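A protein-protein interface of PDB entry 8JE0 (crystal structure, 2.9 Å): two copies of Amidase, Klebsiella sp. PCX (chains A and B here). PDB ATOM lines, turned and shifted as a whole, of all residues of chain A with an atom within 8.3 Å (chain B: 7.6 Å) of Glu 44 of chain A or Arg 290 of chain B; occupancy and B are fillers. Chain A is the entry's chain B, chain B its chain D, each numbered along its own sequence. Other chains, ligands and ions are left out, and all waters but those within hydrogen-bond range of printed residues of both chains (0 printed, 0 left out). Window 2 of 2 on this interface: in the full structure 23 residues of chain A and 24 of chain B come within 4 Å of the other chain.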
ATOM      1  N   LEU A   3      20.045 -37.409 -13.826  1.00  0.00           N
ATOM      2  CA  LEU A   3      18.778 -36.810 -13.419  1.00  0.00           C
ATOM      3  C   LEU A   3      18.422 -35.619 -14.314  1.00  0.00           C
ATOM      4  O   LEU A   3      19.167 -34.641 -14.386  1.00  0.00           O
ATOM      5  CB  LEU A   3      18.852 -36.394 -11.948  1.00  0.00           C
ATOM      6  CG  LEU A   3      17.622 -36.688 -11.094  1.00  0.00           C
ATOM      7  CD1 LEU A   3      17.439 -38.186 -10.977  1.00  0.00           C
ATOM      8  CD2 LEU A   3      17.832 -36.099  -9.721  1.00  0.00           C
ATOM      9  N   ASP A   4      17.270 -35.716 -14.989  1.00  0.00           N
ATOM     10  CA  ASP A   4      16.885 -34.739 -16.005  1.00  0.00           C
ATOM     11  C   ASP A   4      16.276 -33.484 -15.388  1.00  0.00           C
ATOM     12  O   ASP A   4      16.708 -32.369 -15.698  1.00  0.00           O
ATOM     13  CB  ASP A   4      15.905 -35.372 -16.991  1.00  0.00           C
ATOM     14  CG  ASP A   4      16.566 -36.373 -17.903  1.00  0.00           C
ATOM     15  OD1 ASP A   4      17.638 -36.066 -18.473  1.00  0.00           O
ATOM     16  OD2 ASP A   4      16.018 -37.486 -18.027  1.00  0.00           O
ATOM     17  N   ILE A   5      15.270 -33.632 -14.521  1.00  0.00           N
ATOM     18  CA  ILE A   5      14.693 -32.483 -13.833  1.00  0.00           C
ATOM     19  C   ILE A   5      14.669 -32.734 -12.329  1.00  0.00           C
ATOM     20  O   ILE A   5      14.416 -33.838 -11.861  1.00  0.00           O
ATOM     21  CB  ILE A   5      13.273 -32.168 -14.333  1.00  0.00           C
ATOM     22  CG1 ILE A   5      13.295 -31.898 -15.844  1.00  0.00           C
ATOM     23  CG2 ILE A   5      12.712 -30.962 -13.624  1.00  0.00           C
ATOM     24  CD1 ILE A   5      11.944 -32.091 -16.516  1.00  0.00           C
ATOM     25  N   VAL A   6      14.921 -31.685 -11.566  1.00  0.00           N
ATOM     26  CA  VAL A   6      14.665 -31.669 -10.130  1.00  0.00           C
ATOM     27  C   VAL A   6      13.763 -30.492  -9.821  1.00  0.00           C
ATOM     28  O   VAL A   6      14.001 -29.389 -10.327  1.00  0.00           O
ATOM     29  CB  VAL A   6      15.944 -31.599  -9.267  1.00  0.00           C
ATOM     30  CG1 VAL A   6      15.540 -31.279  -7.834  1.00  0.00           C
ATOM     31  CG2 VAL A   6      16.623 -32.911  -9.274  1.00  0.00           C
ATOM     32  N   ILE A  27      13.109 -36.473 -11.452  1.00  0.00           N
ATOM     33  CA  ILE A  27      12.575 -36.896 -12.741  1.00  0.00           C
ATOM     34  C   ILE A  27      13.733 -37.374 -13.601  1.00  0.00           C
ATOM     35  O   ILE A  27      14.694 -36.629 -13.824  1.00  0.00           O
ATOM     36  CB  ILE A  27      11.811 -35.765 -13.447  1.00  0.00           C
ATOM     37  CG1 ILE A  27      10.578 -35.360 -12.638  1.00  0.00           C
ATOM     38  CG2 ILE A  27      11.413 -36.180 -14.851  1.00  0.00           C
ATOM     39  CD1 ILE A  27       9.982 -34.057 -13.096  1.00  0.00           C
ATOM     40  N   LEU A  41      23.142 -35.093  -5.558  1.00  0.00           N
ATOM     41  CA  LEU A  41      22.157 -35.242  -6.625  1.00  0.00           C
ATOM     42  C   LEU A  41      22.184 -34.056  -7.586  1.00  0.00           C
ATOM     43  O   LEU A  41      21.541 -33.035  -7.339  1.00  0.00           O
ATOM     44  CB  LEU A  41      20.752 -35.402  -6.039  1.00  0.00           C
ATOM     45  N   GLN A  42      22.927 -34.192  -8.680  1.00  0.00           N
ATOM     46  CA  GLN A  42      22.978 -33.167  -9.712  1.00  0.00           C
ATOM     47  C   GLN A  42      21.873 -33.398 -10.739  1.00  0.00           C
ATOM     48  O   GLN A  42      21.463 -34.535 -10.991  1.00  0.00           O
ATOM     49  CB  GLN A  42      24.344 -33.158 -10.401  1.00  0.00           C
ATOM     50  N   ALA A  43      21.391 -32.304 -11.331  1.00  0.00           N
ATOM     51  CA  ALA A  43      20.278 -32.363 -12.270  1.00  0.00           C
ATOM     52  C   ALA A  43      20.479 -31.374 -13.408  1.00  0.00           C
ATOM     53  O   ALA A  43      20.929 -30.246 -13.189  1.00  0.00           O
ATOM     54  CB  ALA A  43      18.952 -32.065 -11.578  1.00  0.00           C
ATOM     55  N   GLU A  44      20.104 -31.799 -14.618  1.00  0.00           N
ATOM     56  CA  GLU A  44      20.288 -30.960 -15.799  1.00  0.00           C
ATOM     57  C   GLU A  44      19.436 -29.699 -15.731  1.00  0.00           C
ATOM     58  O   GLU A  44      19.864 -28.628 -16.176  1.00  0.00           O
ATOM     59  CB  GLU A  44      19.965 -31.757 -17.062  1.00  0.00           C
ATOM     60  CG  GLU A  44      20.906 -31.475 -18.224  1.00  0.00           C
ATOM     61  CD  GLU A  44      22.260 -32.145 -18.060  1.00  0.00           C
ATOM     62  OE1 GLU A  44      22.383 -33.334 -18.422  1.00  0.00           O
ATOM     63  OE2 GLU A  44      23.202 -31.482 -17.571  1.00  0.00           O
ATOM     64  N   THR A  45      18.225 -29.806 -15.190  1.00  0.00           N
ATOM     65  CA  THR A  45      17.362 -28.654 -14.967  1.00  0.00           C
ATOM     66  C   THR A  45      16.848 -28.703 -13.536  1.00  0.00           C
ATOM     67  O   THR A  45      16.428 -29.762 -13.060  1.00  0.00           O
ATOM     68  CB  THR A  45      16.189 -28.627 -15.958  1.00  0.00           C
ATOM     69  OG1 THR A  45      16.671 -28.915 -17.275  1.00  0.00           O
ATOM     70  CG2 THR A  45      15.510 -27.260 -15.959  1.00  0.00           C
ATOM     71  N   VAL A  46      16.900 -27.563 -12.852  1.00  0.00           N
ATOM     72  CA  VAL A  46      16.380 -27.425 -11.498  1.00  0.00           C
ATOM     73  C   VAL A  46      15.236 -26.424 -11.538  1.00  0.00           C
ATOM     74  O   VAL A  46      15.392 -25.319 -12.070  1.00  0.00           O
ATOM     75  CB  VAL A  46      17.470 -26.974 -10.506  1.00  0.00           C
ATOM     76  CG1 VAL A  46      16.877 -26.750  -9.126  1.00  0.00           C
ATOM     77  CG2 VAL A  46      18.590 -27.998 -10.441  1.00  0.00           C
ATOM     78  N   ILE A  47      14.086 -26.820 -10.996  1.00  0.00           N
ATOM     79  CA  ILE A  47      12.923 -25.948 -10.882  1.00  0.00           C
ATOM     80  C   ILE A  47      12.827 -25.466  -9.443  1.00  0.00           C
ATOM     81  O   ILE A  47      12.880 -26.272  -8.506  1.00  0.00           O
ATOM     82  CB  ILE A  47      11.631 -26.672 -11.303  1.00  0.00           C
ATOM     83  CG1 ILE A  47      11.809 -27.363 -12.662  1.00  0.00           C
ATOM     84  CG2 ILE A  47      10.449 -25.703 -11.305  1.00  0.00           C
ATOM     85  CD1 ILE A  47      11.412 -26.519 -13.845  1.00  0.00           C
ATOM     86  N   ILE A 380       9.125 -30.377 -19.676  1.00  0.00           N
ATOM     87  CA  ILE A 380       8.636 -29.075 -19.227  1.00  0.00           C
ATOM     88  C   ILE A 380       7.792 -28.492 -20.357  1.00  0.00           C
ATOM     89  O   ILE A 380       8.321 -27.897 -21.295  1.00  0.00           O
ATOM     90  CB  ILE A 380       9.781 -28.140 -18.833  1.00  0.00           C
ATOM     91  CG1 ILE A 380      10.668 -28.802 -17.776  1.00  0.00           C
ATOM     92  CG2 ILE A 380       9.234 -26.813 -18.324  1.00  0.00           C
ATOM     93  CD1 ILE A 380      11.976 -28.086 -17.541  1.00  0.00           C
ATOM     94  N   ARG A 383       6.066 -23.318 -18.081  1.00  0.00           N
ATOM     95  CA  ARG A 383       6.937 -22.844 -17.004  1.00  0.00           C
ATOM     96  C   ARG A 383       7.053 -21.324 -17.111  1.00  0.00           C
ATOM     97  O   ARG A 383       7.774 -20.819 -17.977  1.00  0.00           O
ATOM     98  CB  ARG A 383       8.302 -23.509 -17.079  1.00  0.00           C
ATOM     99  CG  ARG A 383       9.194 -23.252 -15.876  1.00  0.00           C
ATOM    100  CD  ARG A 383      10.631 -23.648 -16.171  1.00  0.00           C
ATOM    101  NE  ARG A 383      11.536 -23.272 -15.091  1.00  0.00           N
ATOM    102  CZ  ARG A 383      12.824 -23.584 -15.052  1.00  0.00           C
ATOM    103  NH1 ARG A 383      13.401 -24.265 -16.029  1.00  0.00           N
ATOM    104  NH2 ARG A 383      13.550 -23.208 -14.004  1.00  0.00           N
ATOM    105  N   LEU A 385       8.503 -17.756 -16.155  1.00  0.00           N
ATOM    106  CA  LEU A 385       9.848 -17.361 -15.750  1.00  0.00           C
ATOM    107  C   LEU A 385       9.914 -17.041 -14.262  1.00  0.00           C
ATOM    108  O   LEU A 385      10.939 -17.287 -13.617  1.00  0.00           O
ATOM    109  CB  LEU A 385      10.306 -16.158 -16.574  1.00  0.00           C
ATOM    110  CG  LEU A 385      10.956 -16.481 -17.919  1.00  0.00           C
ATOM    111  CD1 LEU A 385      11.100 -15.219 -18.762  1.00  0.00           C
ATOM    112  CD2 LEU A 385      12.301 -17.159 -17.716  1.00  0.00           C
ATOM    113  N   VAL B 258      21.385 -22.415 -28.590  1.00  0.00           N
ATOM    114  CA  VAL B 258      22.332 -22.679 -27.520  1.00  0.00           C
ATOM    115  C   VAL B 258      23.768 -22.341 -27.914  1.00  0.00           C
ATOM    116  O   VAL B 258      24.619 -22.181 -27.026  1.00  0.00           O
ATOM    117  CB  VAL B 258      22.206 -24.155 -27.080  1.00  0.00           C
ATOM    118  CG1 VAL B 258      22.835 -25.079 -28.112  1.00  0.00           C
ATOM    119  CG2 VAL B 258      22.793 -24.374 -25.694  1.00  0.00           C
ATOM    120  N   THR B 284      14.378 -25.750 -29.755  1.00  0.00           N
ATOM    121  CA  THR B 284      14.497 -27.199 -29.738  1.00  0.00           C
ATOM    122  C   THR B 284      14.031 -27.726 -28.387  1.00  0.00           C
ATOM    123  O   THR B 284      13.808 -26.966 -27.440  1.00  0.00           O
ATOM    124  CB  THR B 284      15.934 -27.663 -30.015  1.00  0.00           C
ATOM    125  OG1 THR B 284      16.794 -27.251 -28.942  1.00  0.00           O
ATOM    126  CG2 THR B 284      16.444 -27.100 -31.342  1.00  0.00           C
ATOM    127  N   LEU B 285      13.893 -29.051 -28.308  1.00  0.00           N
ATOM    128  CA  LEU B 285      13.488 -29.683 -27.056  1.00  0.00           C
ATOM    129  C   LEU B 285      14.453 -29.357 -25.926  1.00  0.00           C
ATOM    130  O   LEU B 285      14.063 -29.362 -24.752  1.00  0.00           O
ATOM    131  CB  LEU B 285      13.389 -31.196 -27.250  1.00  0.00           C
ATOM    132  CG  LEU B 285      12.637 -32.010 -26.201  1.00  0.00           C
ATOM    133  CD1 LEU B 285      11.284 -31.387 -25.896  1.00  0.00           C
ATOM    134  CD2 LEU B 285      12.475 -33.436 -26.696  1.00  0.00           C
ATOM    135  N   ARG B 286      15.706 -29.054 -26.259  1.00  0.00           N
ATOM    136  CA  ARG B 286      16.733 -28.852 -25.247  1.00  0.00           C
ATOM    137  C   ARG B 286      16.750 -27.422 -24.714  1.00  0.00           C
ATOM    138  O   ARG B 286      17.041 -27.217 -23.531  1.00  0.00           O
ATOM    139  CB  ARG B 286      18.093 -29.240 -25.829  1.00  0.00           C
ATOM    140  CG  ARG B 286      19.273 -28.452 -25.298  1.00  0.00           C
ATOM    141  CD  ARG B 286      20.470 -29.356 -25.068  1.00  0.00           C
ATOM    142  NE  ARG B 286      21.702 -28.596 -24.896  1.00  0.00           N
ATOM    143  CZ  ARG B 286      22.582 -28.375 -25.864  1.00  0.00           C
ATOM    144  NH1 ARG B 286      22.391 -28.838 -27.089  1.00  0.00           N
ATOM    145  NH2 ARG B 286      23.678 -27.672 -25.596  1.00  0.00           N
ATOM    146  N   ASN B 287      16.426 -26.433 -25.548  1.00  0.00           N
ATOM    147  CA  ASN B 287      16.472 -25.031 -25.148  1.00  0.00           C
ATOM    148  C   ASN B 287      15.094 -24.438 -24.871  1.00  0.00           C
ATOM    149  O   ASN B 287      14.991 -23.230 -24.634  1.00  0.00           O
ATOM    150  CB  ASN B 287      17.202 -24.194 -26.210  1.00  0.00           C
ATOM    151  CG  ASN B 287      16.520 -24.225 -27.583  1.00  0.00           C
ATOM    152  OD1 ASN B 287      15.294 -24.291 -27.695  1.00  0.00           O
ATOM    153  ND2 ASN B 287      17.328 -24.164 -28.639  1.00  0.00           N
ATOM    154  N   SER B 288      14.037 -25.245 -24.901  1.00  0.00           N
ATOM    155  CA  SER B 288      12.691 -24.755 -24.634  1.00  0.00           C
ATOM    156  C   SER B 288      12.432 -24.784 -23.133  1.00  0.00           C
ATOM    157  O   SER B 288      12.489 -25.851 -22.511  1.00  0.00           O
ATOM    158  CB  SER B 288      11.641 -25.588 -25.364  1.00  0.00           C
ATOM    159  OG  SER B 288      10.354 -25.369 -24.806  1.00  0.00           O
ATOM    160  N   LEU B 289      12.157 -23.609 -22.558  1.00  0.00           N
ATOM    161  CA  LEU B 289      11.741 -23.490 -21.161  1.00  0.00           C
ATOM    162  C   LEU B 289      12.832 -23.976 -20.209  1.00  0.00           C
ATOM    163  O   LEU B 289      12.547 -24.546 -19.156  1.00  0.00           O
ATOM    164  CB  LEU B 289      10.434 -24.256 -20.918  1.00  0.00           C
ATOM    165  CG  LEU B 289       9.065 -23.567 -21.003  1.00  0.00           C
ATOM    166  CD1 LEU B 289       9.087 -22.333 -21.885  1.00  0.00           C
ATOM    167  CD2 LEU B 289       8.007 -24.549 -21.500  1.00  0.00           C
ATOM    168  N   ARG B 290      14.098 -23.752 -20.569  1.00  0.00           N
ATOM    169  CA  ARG B 290      15.155 -24.420 -19.819  1.00  0.00           C
ATOM    170  C   ARG B 290      16.373 -23.548 -19.534  1.00  0.00           C
ATOM    171  O   ARG B 290      16.633 -23.202 -18.375  1.00  0.00           O
ATOM    172  CB  ARG B 290      15.581 -25.686 -20.559  1.00  0.00           C
ATOM    173  CG  ARG B 290      15.665 -26.899 -19.656  1.00  0.00           C
ATOM    174  CD  ARG B 290      16.325 -28.058 -20.362  1.00  0.00           C
ATOM    175  NE  ARG B 290      17.609 -27.668 -20.929  1.00  0.00           N
ATOM    176  CZ  ARG B 290      18.781 -27.917 -20.365  1.00  0.00           C
ATOM    177  NH1 ARG B 290      18.870 -28.551 -19.206  1.00  0.00           N
ATOM    178  NH2 ARG B 290      19.893 -27.518 -20.976  1.00  0.00           N
ATOM    179  N   THR B 291      17.143 -23.204 -20.562  1.00  0.00           N
ATOM    180  CA  THR B 291      18.403 -22.516 -20.327  1.00  0.00           C
ATOM    181  C   THR B 291      18.156 -21.060 -19.941  1.00  0.00           C
ATOM    182  O   THR B 291      17.019 -20.610 -19.768  1.00  0.00           O
ATOM    183  CB  THR B 291      19.294 -22.589 -21.564  1.00  0.00           C
ATOM    184  OG1 THR B 291      18.802 -21.686 -22.563  1.00  0.00           O
ATOM    185  CG2 THR B 291      19.320 -24.002 -22.119  1.00  0.00           C
ATOM    186  N   ASP B 292      19.251 -20.315 -19.796  1.00  0.00           N
ATOM    187  CA  ASP B 292      19.208 -18.863 -19.710  1.00  0.00           C
ATOM    188  C   ASP B 292      19.582 -18.209 -21.036  1.00  0.00           C
ATOM    189  O   ASP B 292      19.853 -17.003 -21.076  1.00  0.00           O
ATOM    190  CB  ASP B 292      20.121 -18.370 -18.586  1.00  0.00           C
ATOM    191  N   LYS B 293      19.601 -18.984 -22.121  1.00  0.00           N
ATOM    192  CA  LYS B 293      19.966 -18.491 -23.443  1.00  0.00           C
ATOM    193  C   LYS B 293      18.716 -18.361 -24.306  1.00  0.00           C
ATOM    194  O   LYS B 293      18.220 -17.253 -24.538  1.00  0.00           O
ATOM    195  CB  LYS B 293      20.990 -19.426 -24.089  1.00  0.00           C
ATOM    196  N   VAL B 294      18.214 -19.484 -24.796  1.00  0.00           N
ATOM    197  CA  VAL B 294      16.850 -19.555 -25.287  1.00  0.00           C
ATOM    198  C   VAL B 294      15.971 -20.034 -24.139  1.00  0.00           C
ATOM    199  O   VAL B 294      16.435 -20.670 -23.190  1.00  0.00           O
ATOM    200  CB  VAL B 294      16.721 -20.480 -26.515  1.00  0.00           C
ATOM    201  N   TYR B 295      14.685 -19.715 -24.216  1.00  0.00           N
ATOM    202  CA  TYR B 295      13.739 -20.181 -23.211  1.00  0.00           C
ATOM    203  C   TYR B 295      12.347 -20.125 -23.813  1.00  0.00           C
ATOM    204  O   TYR B 295      11.507 -20.996 -23.577  1.00  0.00           O
ATOM    205  CB  TYR B 295      13.831 -19.324 -21.944  1.00  0.00           C
ATOM    206  CG  TYR B 295      12.890 -19.729 -20.826  1.00  0.00           C
ATOM    207  CD1 TYR B 295      11.579 -19.274 -20.796  1.00  0.00           C
ATOM    208  CD2 TYR B 295      13.323 -20.549 -19.790  1.00  0.00           C
ATOM    209  CE1 TYR B 295      10.719 -19.636 -19.777  1.00  0.00           C
ATOM    210  CE2 TYR B 295      12.468 -20.914 -18.762  1.00  0.00           C
ATOM    211  CZ  TYR B 295      11.168 -20.452 -18.763  1.00  0.00           C
ATOM    212  OH  TYR B 295      10.308 -20.809 -17.752  1.00  0.00           O
ATOM    213  N   SER B 296      12.124 -19.088 -24.608  1.00  0.00           N
ATOM    214  CA  SER B 296      10.877 -18.779 -25.278  1.00  0.00           C
ATOM    215  C   SER B 296      11.175 -17.567 -26.142  1.00  0.00           C
ATOM    216  O   SER B 296      12.208 -16.913 -25.968  1.00  0.00           O
ATOM    217  CB  SER B 296       9.745 -18.486 -24.291  1.00  0.00           C
ATOM    218  OG  SER B 296       9.827 -17.157 -23.805  1.00  0.00           O
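Among the printed residues, merely in contact across the chains: Ile 380 of chain A with Leu 289 of chain B (3.4 Å) and Leu 385 of chain A with Tyr 295 of chain B (3.6 Å).
Printed residues of chain A that touch a printed residue of chain B: Glu 44, Thr 45, Ile 380, Arg 383 and Leu 385. Hydrophobic or aromatic side chains of chain A that line the printed part of chain B: Ile 380 and Leu 385. Along chain A the printed residues that touch a printed residue of chain B span positions 44 to 385.
No position is printed for both chains. Of the 6 pairs that touch across the chains among the printed residues, none has its exchanged pair printed and touching as well.
The backbone NH (N) of Glu 44 of chain A sits at hydrogen-bond distance from the backbone carbonyl oxygen (O) of Leu 3 of chain A. O of Asp 4 of chain A lies within hydrogen-bond range of N of Thr 45 of chain A (3.0 Å). The backbone carbonyl oxygen of Thr 45 of chain A is in hydrogen-bond range of the backbone NH of Val 6 of chain A (2.9 Å). The backbone carbonyl oxygen of Val 46 of chain A sits at hydrogen-bond distance from the guanidinium group of Arg 383 of chain A (3.4 Å). The guanidinium group (NE) of Arg 290 of chain B is in hydrogen-bond range of the backbone carbonyl oxygen (O) of Arg 286 of chain B (2.7 Å). O of Tyr 295 of chain B lies within hydrogen-bond range of N of Leu 289 of chain B (2.9 Å).
Glu 44 of chain A touches just one residue of chain B: Arg 290 (3.2 Å). Of the printed residues of chain B, Ile 380 of chain A touches Leu 289. Printed residues of chain B within 4 Å of Arg 383 of chain A: Leu 289 and Tyr 295. Of the printed residues of chain B, Leu 385 of chain A touches Tyr 295. Val 294 of chain B touches none of the printed residues of chain A. Of the printed residues of chain A, Tyr 295 of chain B touches Arg 383 and Leu 385. The nearest residue of chain B that does not touch Glu 44 of chain A is Arg 286 of chain B (7.2 Å).
The backbone carbonyl oxygen (O) of Glu 44 of chain A sits at hydrogen-bond distance from the guanidinium group (NH1) of Arg 290 of chain B, at 3.2 Å. The side-chain hydroxyl (OG1) of Thr 45 of chain A sits at hydrogen-bond distance from the guanidinium group (NH1) of Arg 290 of chain B, at 2.9 Å. NH1 of Arg 383 of chain A lies within hydrogen-bond range of O of Leu 289 of chain B (3.3 Å). OH of Tyr 295 of chain B is in hydrogen-bond range of O of Arg 383 of chain A (2.5 Å).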
